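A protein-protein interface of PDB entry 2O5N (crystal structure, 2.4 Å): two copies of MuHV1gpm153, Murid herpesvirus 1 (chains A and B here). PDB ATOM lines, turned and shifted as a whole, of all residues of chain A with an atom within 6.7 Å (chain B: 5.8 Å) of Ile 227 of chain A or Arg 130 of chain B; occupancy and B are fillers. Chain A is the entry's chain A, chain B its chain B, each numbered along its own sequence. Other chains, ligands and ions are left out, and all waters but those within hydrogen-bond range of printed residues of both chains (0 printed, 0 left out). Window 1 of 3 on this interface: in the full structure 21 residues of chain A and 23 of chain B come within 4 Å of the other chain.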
ATOM      1  N   HIS A 214       4.386  -9.846 -26.425  1.00  0.00           N
ATOM      2  CA  HIS A 214       5.062  -8.703 -25.855  1.00  0.00           C
ATOM      3  C   HIS A 214       4.236  -7.468 -26.209  1.00  0.00           C
ATOM      4  O   HIS A 214       4.152  -7.079 -27.376  1.00  0.00           O
ATOM      5  CB  HIS A 214       6.477  -8.599 -26.438  1.00  0.00           C
ATOM      6  CG  HIS A 214       7.303  -7.499 -25.843  1.00  0.00           C
ATOM      7  ND1 HIS A 214       7.032  -6.163 -26.053  1.00  0.00           N
ATOM      8  CD2 HIS A 214       8.402  -7.542 -25.051  1.00  0.00           C
ATOM      9  CE1 HIS A 214       7.923  -5.430 -25.408  1.00  0.00           C
ATOM     10  NE2 HIS A 214       8.763  -6.241 -24.788  1.00  0.00           N
ATOM     11  N   MET A 215       3.615  -6.876 -25.190  1.00  0.00           N
ATOM     12  CA  MET A 215       2.789  -5.690 -25.338  1.00  0.00           C
ATOM     13  C   MET A 215       3.473  -4.442 -24.774  1.00  0.00           C
ATOM     14  O   MET A 215       3.916  -4.437 -23.619  1.00  0.00           O
ATOM     15  CB  MET A 215       1.456  -5.899 -24.633  1.00  0.00           C
ATOM     16  CG  MET A 215       0.621  -4.644 -24.523  1.00  0.00           C
ATOM     17  SD  MET A 215      -1.044  -4.992 -23.626  1.00  0.00           S
ATOM     18  CE  MET A 215      -1.883  -6.201 -24.928  1.00  0.00           C
ATOM     19  N   THR A 216       3.552  -3.397 -25.602  1.00  0.00           N
ATOM     20  CA  THR A 216       4.078  -2.092 -25.211  1.00  0.00           C
ATOM     21  C   THR A 216       3.042  -1.013 -25.467  1.00  0.00           C
ATOM     22  O   THR A 216       2.513  -0.907 -26.567  1.00  0.00           O
ATOM     23  CB  THR A 216       5.348  -1.709 -26.000  1.00  0.00           C
ATOM     24  OG1 THR A 216       6.262  -2.807 -26.008  1.00  0.00           O
ATOM     25  CG2 THR A 216       6.020  -0.477 -25.378  1.00  0.00           C
ATOM     26  N   VAL A 217       2.761  -0.211 -24.448  1.00  0.00           N
ATOM     27  CA  VAL A 217       1.880   0.936 -24.589  1.00  0.00           C
ATOM     28  C   VAL A 217       2.782   2.173 -24.608  1.00  0.00           C
ATOM     29  O   VAL A 217       3.507   2.441 -23.648  1.00  0.00           O
ATOM     30  CB  VAL A 217       0.819   1.006 -23.442  1.00  0.00           C
ATOM     31  CG1 VAL A 217      -0.192   2.128 -23.690  1.00  0.00           C
ATOM     32  CG2 VAL A 217       0.093  -0.318 -23.286  1.00  0.00           C
ATOM     33  N   ARG A 225       6.700   4.446 -21.765  1.00  0.00           N
ATOM     34  CA  ARG A 225       6.108   3.188 -22.206  1.00  0.00           C
ATOM     35  C   ARG A 225       5.794   2.245 -21.041  1.00  0.00           C
ATOM     36  O   ARG A 225       6.410   2.341 -19.982  1.00  0.00           O
ATOM     37  CB  ARG A 225       7.035   2.484 -23.205  1.00  0.00           C
ATOM     38  CG  ARG A 225       8.375   2.015 -22.621  1.00  0.00           C
ATOM     39  CD  ARG A 225       9.052   1.029 -23.552  1.00  0.00           C
ATOM     40  NE  ARG A 225      10.496   0.961 -23.340  1.00  0.00           N
ATOM     41  CZ  ARG A 225      11.347   0.286 -24.114  1.00  0.00           C
ATOM     42  NH1 ARG A 225      10.916  -0.403 -25.168  1.00  0.00           N
ATOM     43  NH2 ARG A 225      12.641   0.294 -23.830  1.00  0.00           N
ATOM     44  N   ALA A 226       4.833   1.342 -21.251  1.00  0.00           N
ATOM     45  CA  ALA A 226       4.568   0.241 -20.323  1.00  0.00           C
ATOM     46  C   ALA A 226       4.672  -1.077 -21.063  1.00  0.00           C
ATOM     47  O   ALA A 226       4.212  -1.198 -22.192  1.00  0.00           O
ATOM     48  CB  ALA A 226       3.225   0.384 -19.690  1.00  0.00           C
ATOM     49  N   ILE A 227       5.313  -2.055 -20.438  1.00  0.00           N
ATOM     50  CA  ILE A 227       5.584  -3.334 -21.078  1.00  0.00           C
ATOM     51  C   ILE A 227       4.964  -4.466 -20.269  1.00  0.00           C
ATOM     52  O   ILE A 227       5.124  -4.533 -19.048  1.00  0.00           O
ATOM     53  CB  ILE A 227       7.111  -3.581 -21.310  1.00  0.00           C
ATOM     54  CG1 ILE A 227       7.703  -2.529 -22.266  1.00  0.00           C
ATOM     55  CG2 ILE A 227       7.360  -4.988 -21.861  1.00  0.00           C
ATOM     56  CD1 ILE A 227       9.215  -2.693 -22.549  1.00  0.00           C
ATOM     57  N   ALA A 228       4.232  -5.330 -20.970  1.00  0.00           N
ATOM     58  CA  ALA A 228       3.667  -6.532 -20.377  1.00  0.00           C
ATOM     59  C   ALA A 228       4.044  -7.752 -21.217  1.00  0.00           C
ATOM     60  O   ALA A 228       4.393  -7.629 -22.394  1.00  0.00           O
ATOM     61  CB  ALA A 228       2.161  -6.404 -20.237  1.00  0.00           C
ATOM     62  N   LEU A 229       4.019  -8.924 -20.588  1.00  0.00           N
ATOM     63  CA  LEU A 229       4.163 -10.186 -21.311  1.00  0.00           C
ATOM     64  C   LEU A 229       2.974 -11.057 -20.980  1.00  0.00           C
ATOM     65  O   LEU A 229       2.384 -10.920 -19.915  1.00  0.00           O
ATOM     66  CB  LEU A 229       5.461 -10.908 -20.963  1.00  0.00           C
ATOM     67  CG  LEU A 229       6.789 -10.144 -20.976  1.00  0.00           C
ATOM     68  CD1 LEU A 229       7.879 -11.087 -20.506  1.00  0.00           C
ATOM     69  CD2 LEU A 229       7.152  -9.579 -22.335  1.00  0.00           C
ATOM     70  N   ALA A 240      -2.260  -7.670 -20.696  1.00  0.00           N
ATOM     71  CA  ALA A 240      -2.725  -6.343 -20.331  1.00  0.00           C
ATOM     72  C   ALA A 240      -1.588  -5.468 -19.822  1.00  0.00           C
ATOM     73  O   ALA A 240      -0.643  -5.958 -19.206  1.00  0.00           O
ATOM     74  CB  ALA A 240      -3.861  -6.425 -19.312  1.00  0.00           C
ATOM     75  N   SER A 241      -1.698  -4.171 -20.104  1.00  0.00           N
ATOM     76  CA  SER A 241      -0.665  -3.200 -19.791  1.00  0.00           C
ATOM     77  C   SER A 241      -1.321  -1.848 -19.555  1.00  0.00           C
ATOM     78  O   SER A 241      -2.346  -1.546 -20.157  1.00  0.00           O
ATOM     79  CB  SER A 241       0.367  -3.117 -20.927  1.00  0.00           C
ATOM     80  OG  SER A 241       1.467  -2.306 -20.571  1.00  0.00           O
ATOM     81  N   TYR A 242      -0.712  -1.051 -18.675  1.00  0.00           N
ATOM     82  CA  TYR A 242      -1.327   0.165 -18.144  1.00  0.00           C
ATOM     83  C   TYR A 242      -0.327   1.338 -18.130  1.00  0.00           C
ATOM     84  O   TYR A 242       0.720   1.276 -17.470  1.00  0.00           O
ATOM     85  CB  TYR A 242      -1.868  -0.083 -16.722  1.00  0.00           C
ATOM     86  CG  TYR A 242      -2.705  -1.346 -16.538  1.00  0.00           C
ATOM     87  CD1 TYR A 242      -4.103  -1.290 -16.485  1.00  0.00           C
ATOM     88  CD2 TYR A 242      -2.094  -2.599 -16.393  1.00  0.00           C
ATOM     89  CE1 TYR A 242      -4.873  -2.464 -16.306  1.00  0.00           C
ATOM     90  CE2 TYR A 242      -2.843  -3.765 -16.231  1.00  0.00           C
ATOM     91  CZ  TYR A 242      -4.230  -3.698 -16.186  1.00  0.00           C
ATOM     92  OH  TYR A 242      -4.956  -4.871 -16.010  1.00  0.00           O
ATOM     93  N   GLU B 117      13.686  -8.013  -9.017  1.00  0.00           N
ATOM     94  CA  GLU B 117      13.146  -7.887 -10.378  1.00  0.00           C
ATOM     95  C   GLU B 117      12.884  -6.433 -10.799  1.00  0.00           C
ATOM     96  O   GLU B 117      12.240  -5.665 -10.063  1.00  0.00           O
ATOM     97  CB  GLU B 117      11.879  -8.749 -10.552  1.00  0.00           C
ATOM     98  N   THR B 118      13.397  -6.071 -11.977  1.00  0.00           N
ATOM     99  CA  THR B 118      13.208  -4.742 -12.559  1.00  0.00           C
ATOM    100  C   THR B 118      11.733  -4.423 -12.792  1.00  0.00           C
ATOM    101  O   THR B 118      11.051  -5.150 -13.513  1.00  0.00           O
ATOM    102  CB  THR B 118      13.975  -4.586 -13.902  1.00  0.00           C
ATOM    103  OG1 THR B 118      15.360  -4.881 -13.701  1.00  0.00           O
ATOM    104  CG2 THR B 118      13.868  -3.153 -14.420  1.00  0.00           C
ATOM    105  N   ILE B 119      11.262  -3.333 -12.184  1.00  0.00           N
ATOM    106  CA  ILE B 119       9.884  -2.850 -12.334  1.00  0.00           C
ATOM    107  C   ILE B 119       9.777  -1.513 -13.105  1.00  0.00           C
ATOM    108  O   ILE B 119       8.731  -1.201 -13.676  1.00  0.00           O
ATOM    109  CB  ILE B 119       9.153  -2.724 -10.945  1.00  0.00           C
ATOM    110  CG1 ILE B 119       9.887  -1.736 -10.021  1.00  0.00           C
ATOM    111  CG2 ILE B 119       9.005  -4.104 -10.277  1.00  0.00           C
ATOM    112  CD1 ILE B 119       9.071  -1.209  -8.838  1.00  0.00           C
ATOM    113  N   MET B 120      10.846  -0.717 -13.092  1.00  0.00           N
ATOM    114  CA  MET B 120      10.851   0.596 -13.757  1.00  0.00           C
ATOM    115  C   MET B 120      12.256   1.011 -14.153  1.00  0.00           C
ATOM    116  O   MET B 120      13.227   0.579 -13.541  1.00  0.00           O
ATOM    117  CB  MET B 120      10.273   1.684 -12.855  1.00  0.00           C
ATOM    118  CG  MET B 120       8.777   1.631 -12.602  1.00  0.00           C
ATOM    119  SD  MET B 120       8.267   3.112 -11.458  1.00  0.00           S
ATOM    120  CE  MET B 120       7.372   4.234 -12.731  1.00  0.00           C
ATOM    121  N   THR B 128      10.323   3.648 -18.678  1.00  0.00           N
ATOM    122  CA  THR B 128       9.711   2.323 -18.833  1.00  0.00           C
ATOM    123  C   THR B 128       9.124   1.850 -17.496  1.00  0.00           C
ATOM    124  O   THR B 128       9.784   1.916 -16.460  1.00  0.00           O
ATOM    125  CB  THR B 128      10.735   1.274 -19.359  1.00  0.00           C
ATOM    126  OG1 THR B 128      11.296   1.707 -20.609  1.00  0.00           O
ATOM    127  CG2 THR B 128      10.097  -0.108 -19.544  1.00  0.00           C
ATOM    128  N   ILE B 129       7.871   1.399 -17.533  1.00  0.00           N
ATOM    129  CA  ILE B 129       7.272   0.631 -16.442  1.00  0.00           C
ATOM    130  C   ILE B 129       7.038  -0.793 -16.962  1.00  0.00           C
ATOM    131  O   ILE B 129       6.537  -0.979 -18.067  1.00  0.00           O
ATOM    132  CB  ILE B 129       5.933   1.256 -15.942  1.00  0.00           C
ATOM    133  CG1 ILE B 129       6.150   2.686 -15.432  1.00  0.00           C
ATOM    134  CG2 ILE B 129       5.309   0.424 -14.820  1.00  0.00           C
ATOM    135  CD1 ILE B 129       4.861   3.446 -15.053  1.00  0.00           C
ATOM    136  N   ARG B 130       7.443  -1.801 -16.198  1.00  0.00           N
ATOM    137  CA  ARG B 130       7.002  -3.157 -16.490  1.00  0.00           C
ATOM    138  C   ARG B 130       5.739  -3.375 -15.663  1.00  0.00           C
ATOM    139  O   ARG B 130       5.723  -3.083 -14.466  1.00  0.00           O
ATOM    140  CB  ARG B 130       8.101  -4.191 -16.207  1.00  0.00           C
ATOM    141  CG  ARG B 130       7.600  -5.618 -15.942  1.00  0.00           C
ATOM    142  CD  ARG B 130       8.360  -6.683 -16.734  1.00  0.00           C
ATOM    143  NE  ARG B 130       9.800  -6.735 -16.442  1.00  0.00           N
ATOM    144  CZ  ARG B 130      10.375  -7.598 -15.604  1.00  0.00           C
ATOM    145  NH1 ARG B 130       9.644  -8.497 -14.946  1.00  0.00           N
ATOM    146  NH2 ARG B 130      11.690  -7.563 -15.423  1.00  0.00           N
ATOM    147  N   SER B 131       4.680  -3.861 -16.313  1.00  0.00           N
ATOM    148  CA  SER B 131       3.357  -3.945 -15.691  1.00  0.00           C
ATOM    149  C   SER B 131       3.148  -5.152 -14.753  1.00  0.00           C
ATOM    150  O   SER B 131       2.435  -6.107 -15.072  1.00  0.00           O
ATOM    151  CB  SER B 131       2.260  -3.829 -16.754  1.00  0.00           C
ATOM    152  OG  SER B 131       2.159  -2.487 -17.201  1.00  0.00           O
ATOM    153  N   VAL B 132       3.787  -5.077 -13.589  1.00  0.00           N
ATOM    154  CA  VAL B 132       3.677  -6.080 -12.533  1.00  0.00           C
ATOM    155  C   VAL B 132       3.222  -5.406 -11.234  1.00  0.00           C
ATOM    156  O   VAL B 132       3.338  -5.974 -10.150  1.00  0.00           O
ATOM    157  CB  VAL B 132       5.007  -6.859 -12.326  1.00  0.00           C
ATOM    158  CG1 VAL B 132       5.171  -7.921 -13.391  1.00  0.00           C
ATOM    159  CG2 VAL B 132       6.221  -5.921 -12.305  1.00  0.00           C
ATOM    160  N   THR B 133       2.681  -4.193 -11.379  1.00  0.00           N
ATOM    161  CA  THR B 133       2.259  -3.337 -10.273  1.00  0.00           C
ATOM    162  C   THR B 133       1.398  -4.094  -9.269  1.00  0.00           C
ATOM    163  O   THR B 133       1.676  -4.083  -8.066  1.00  0.00           O
ATOM    164  CB  THR B 133       1.484  -2.109 -10.798  1.00  0.00           C
ATOM    165  OG1 THR B 133       2.158  -1.567 -11.942  1.00  0.00           O
ATOM    166  CG2 THR B 133       1.368  -1.030  -9.726  1.00  0.00           C
ATOM    167  N   TYR B 136       3.014  -5.869  -6.073  1.00  0.00           N
ATOM    168  CA  TYR B 136       3.646  -5.156  -4.959  1.00  0.00           C
ATOM    169  C   TYR B 136       2.858  -3.926  -4.466  1.00  0.00           C
ATOM    170  O   TYR B 136       3.102  -3.437  -3.361  1.00  0.00           O
ATOM    171  CB  TYR B 136       5.098  -4.779  -5.299  1.00  0.00           C
ATOM    172  CG  TYR B 136       5.260  -3.834  -6.475  1.00  0.00           C
ATOM    173  CD1 TYR B 136       5.407  -4.322  -7.779  1.00  0.00           C
ATOM    174  CD2 TYR B 136       5.285  -2.458  -6.284  1.00  0.00           C
ATOM    175  CE1 TYR B 136       5.559  -3.461  -8.858  1.00  0.00           C
ATOM    176  CE2 TYR B 136       5.436  -1.587  -7.356  1.00  0.00           C
ATOM    177  CZ  TYR B 136       5.569  -2.093  -8.638  1.00  0.00           C
ATOM    178  OH  TYR B 136       5.722  -1.223  -9.689  1.00  0.00           O
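Of the printed residues of chain B, Ala 226 of chain A touches Ile 129 and Ser 131. Ile 227 of chain A touches just these residues of chain B: Ile 129, Arg 130 and Ser 131. Printed residues of chain B within 4 Å of Tyr 242 of chain A: Ser 131 (3.5 Å). Of the printed residues of chain A, Thr 128 of chain B touches Arg 225 (2.9 Å). Of the printed residues of chain A, Ile 129 of chain B touches Arg 225, Ala 226 and Ile 227. Of chain A, only Ile 227 comes within 4 Å of Arg 130 of chain B. Of the printed residues of chain A, Ser 131 of chain B touches Ala 226, Ile 227, Ser 241 and Tyr 242. The nearest residue of chain B that does not touch Ile 227 of chain A is Thr 128 of chain B (4.1 Å). The nearest residue of chain A that does not touch Arg 130 of chain B is Ala 226 of chain A (5.4 Å).
No position is printed for both chains.
The backbone NH (N) of Ser 241 of chain A lies close to the side-chain sulfur (SD) of Met 215 of chain A, at 3.7 Å. The backbone NH of Val 217 of chain A sits at hydrogen-bond distance from the backbone carbonyl oxygen of Ala 226 of chain A (2.9 Å). The backbone carbonyl oxygen (O) of Ala 226 of chain A sits close to the side-chain hydroxyl (OG) of Ser 241 of chain A (3.4 Å). The guanidinium group of Arg 130 of chain B is in hydrogen-bond range of the backbone carbonyl oxygen of Thr 118 of chain B (3.1 Å). The backbone NH of Arg 130 of chain B is in hydrogen-bond range of the backbone carbonyl oxygen of Ile 119 of chain B, 2.9 Å away.
Among the printed residues, merely in contact across the chains: Ala 226 of chain A with Ile 129 of chain B (3.2 Å), Ala 226 of chain A with Ser 131 of chain B (3.9 Å), Ile 227 of chain A with Arg 130 of chain B (3.5 Å) and Tyr 242 of chain A with Ser 131 of chain B (3.5 Å).
OG1 of Thr 128 of chain B sits at hydrogen-bond distance from NE of Arg 225 of chain A, at 2.9 Å. N of Ile 129 of chain B is in hydrogen-bond range of O of Arg 225 of chain A, 3.0 Å away. N of Ile 227 of chain A is in hydrogen-bond range of O of Ile 129 of chain B (2.9 Å). The backbone carbonyl oxygen (O) of Ile 227 of chain A sits at hydrogen-bond distance from the backbone NH (N) of Ser 131 of chain B, at 2.9 Å. The side-chain hydroxyl of Ser 131 of chain B is in hydrogen-bond range of the side-chain hydroxyl of Ser 241 of chain A (3.4 Å).
Printed residues of chain A that touch a printed residue of chain B: Arg 225, Ala 226, Ile 227, Ser 241 and Tyr 242.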
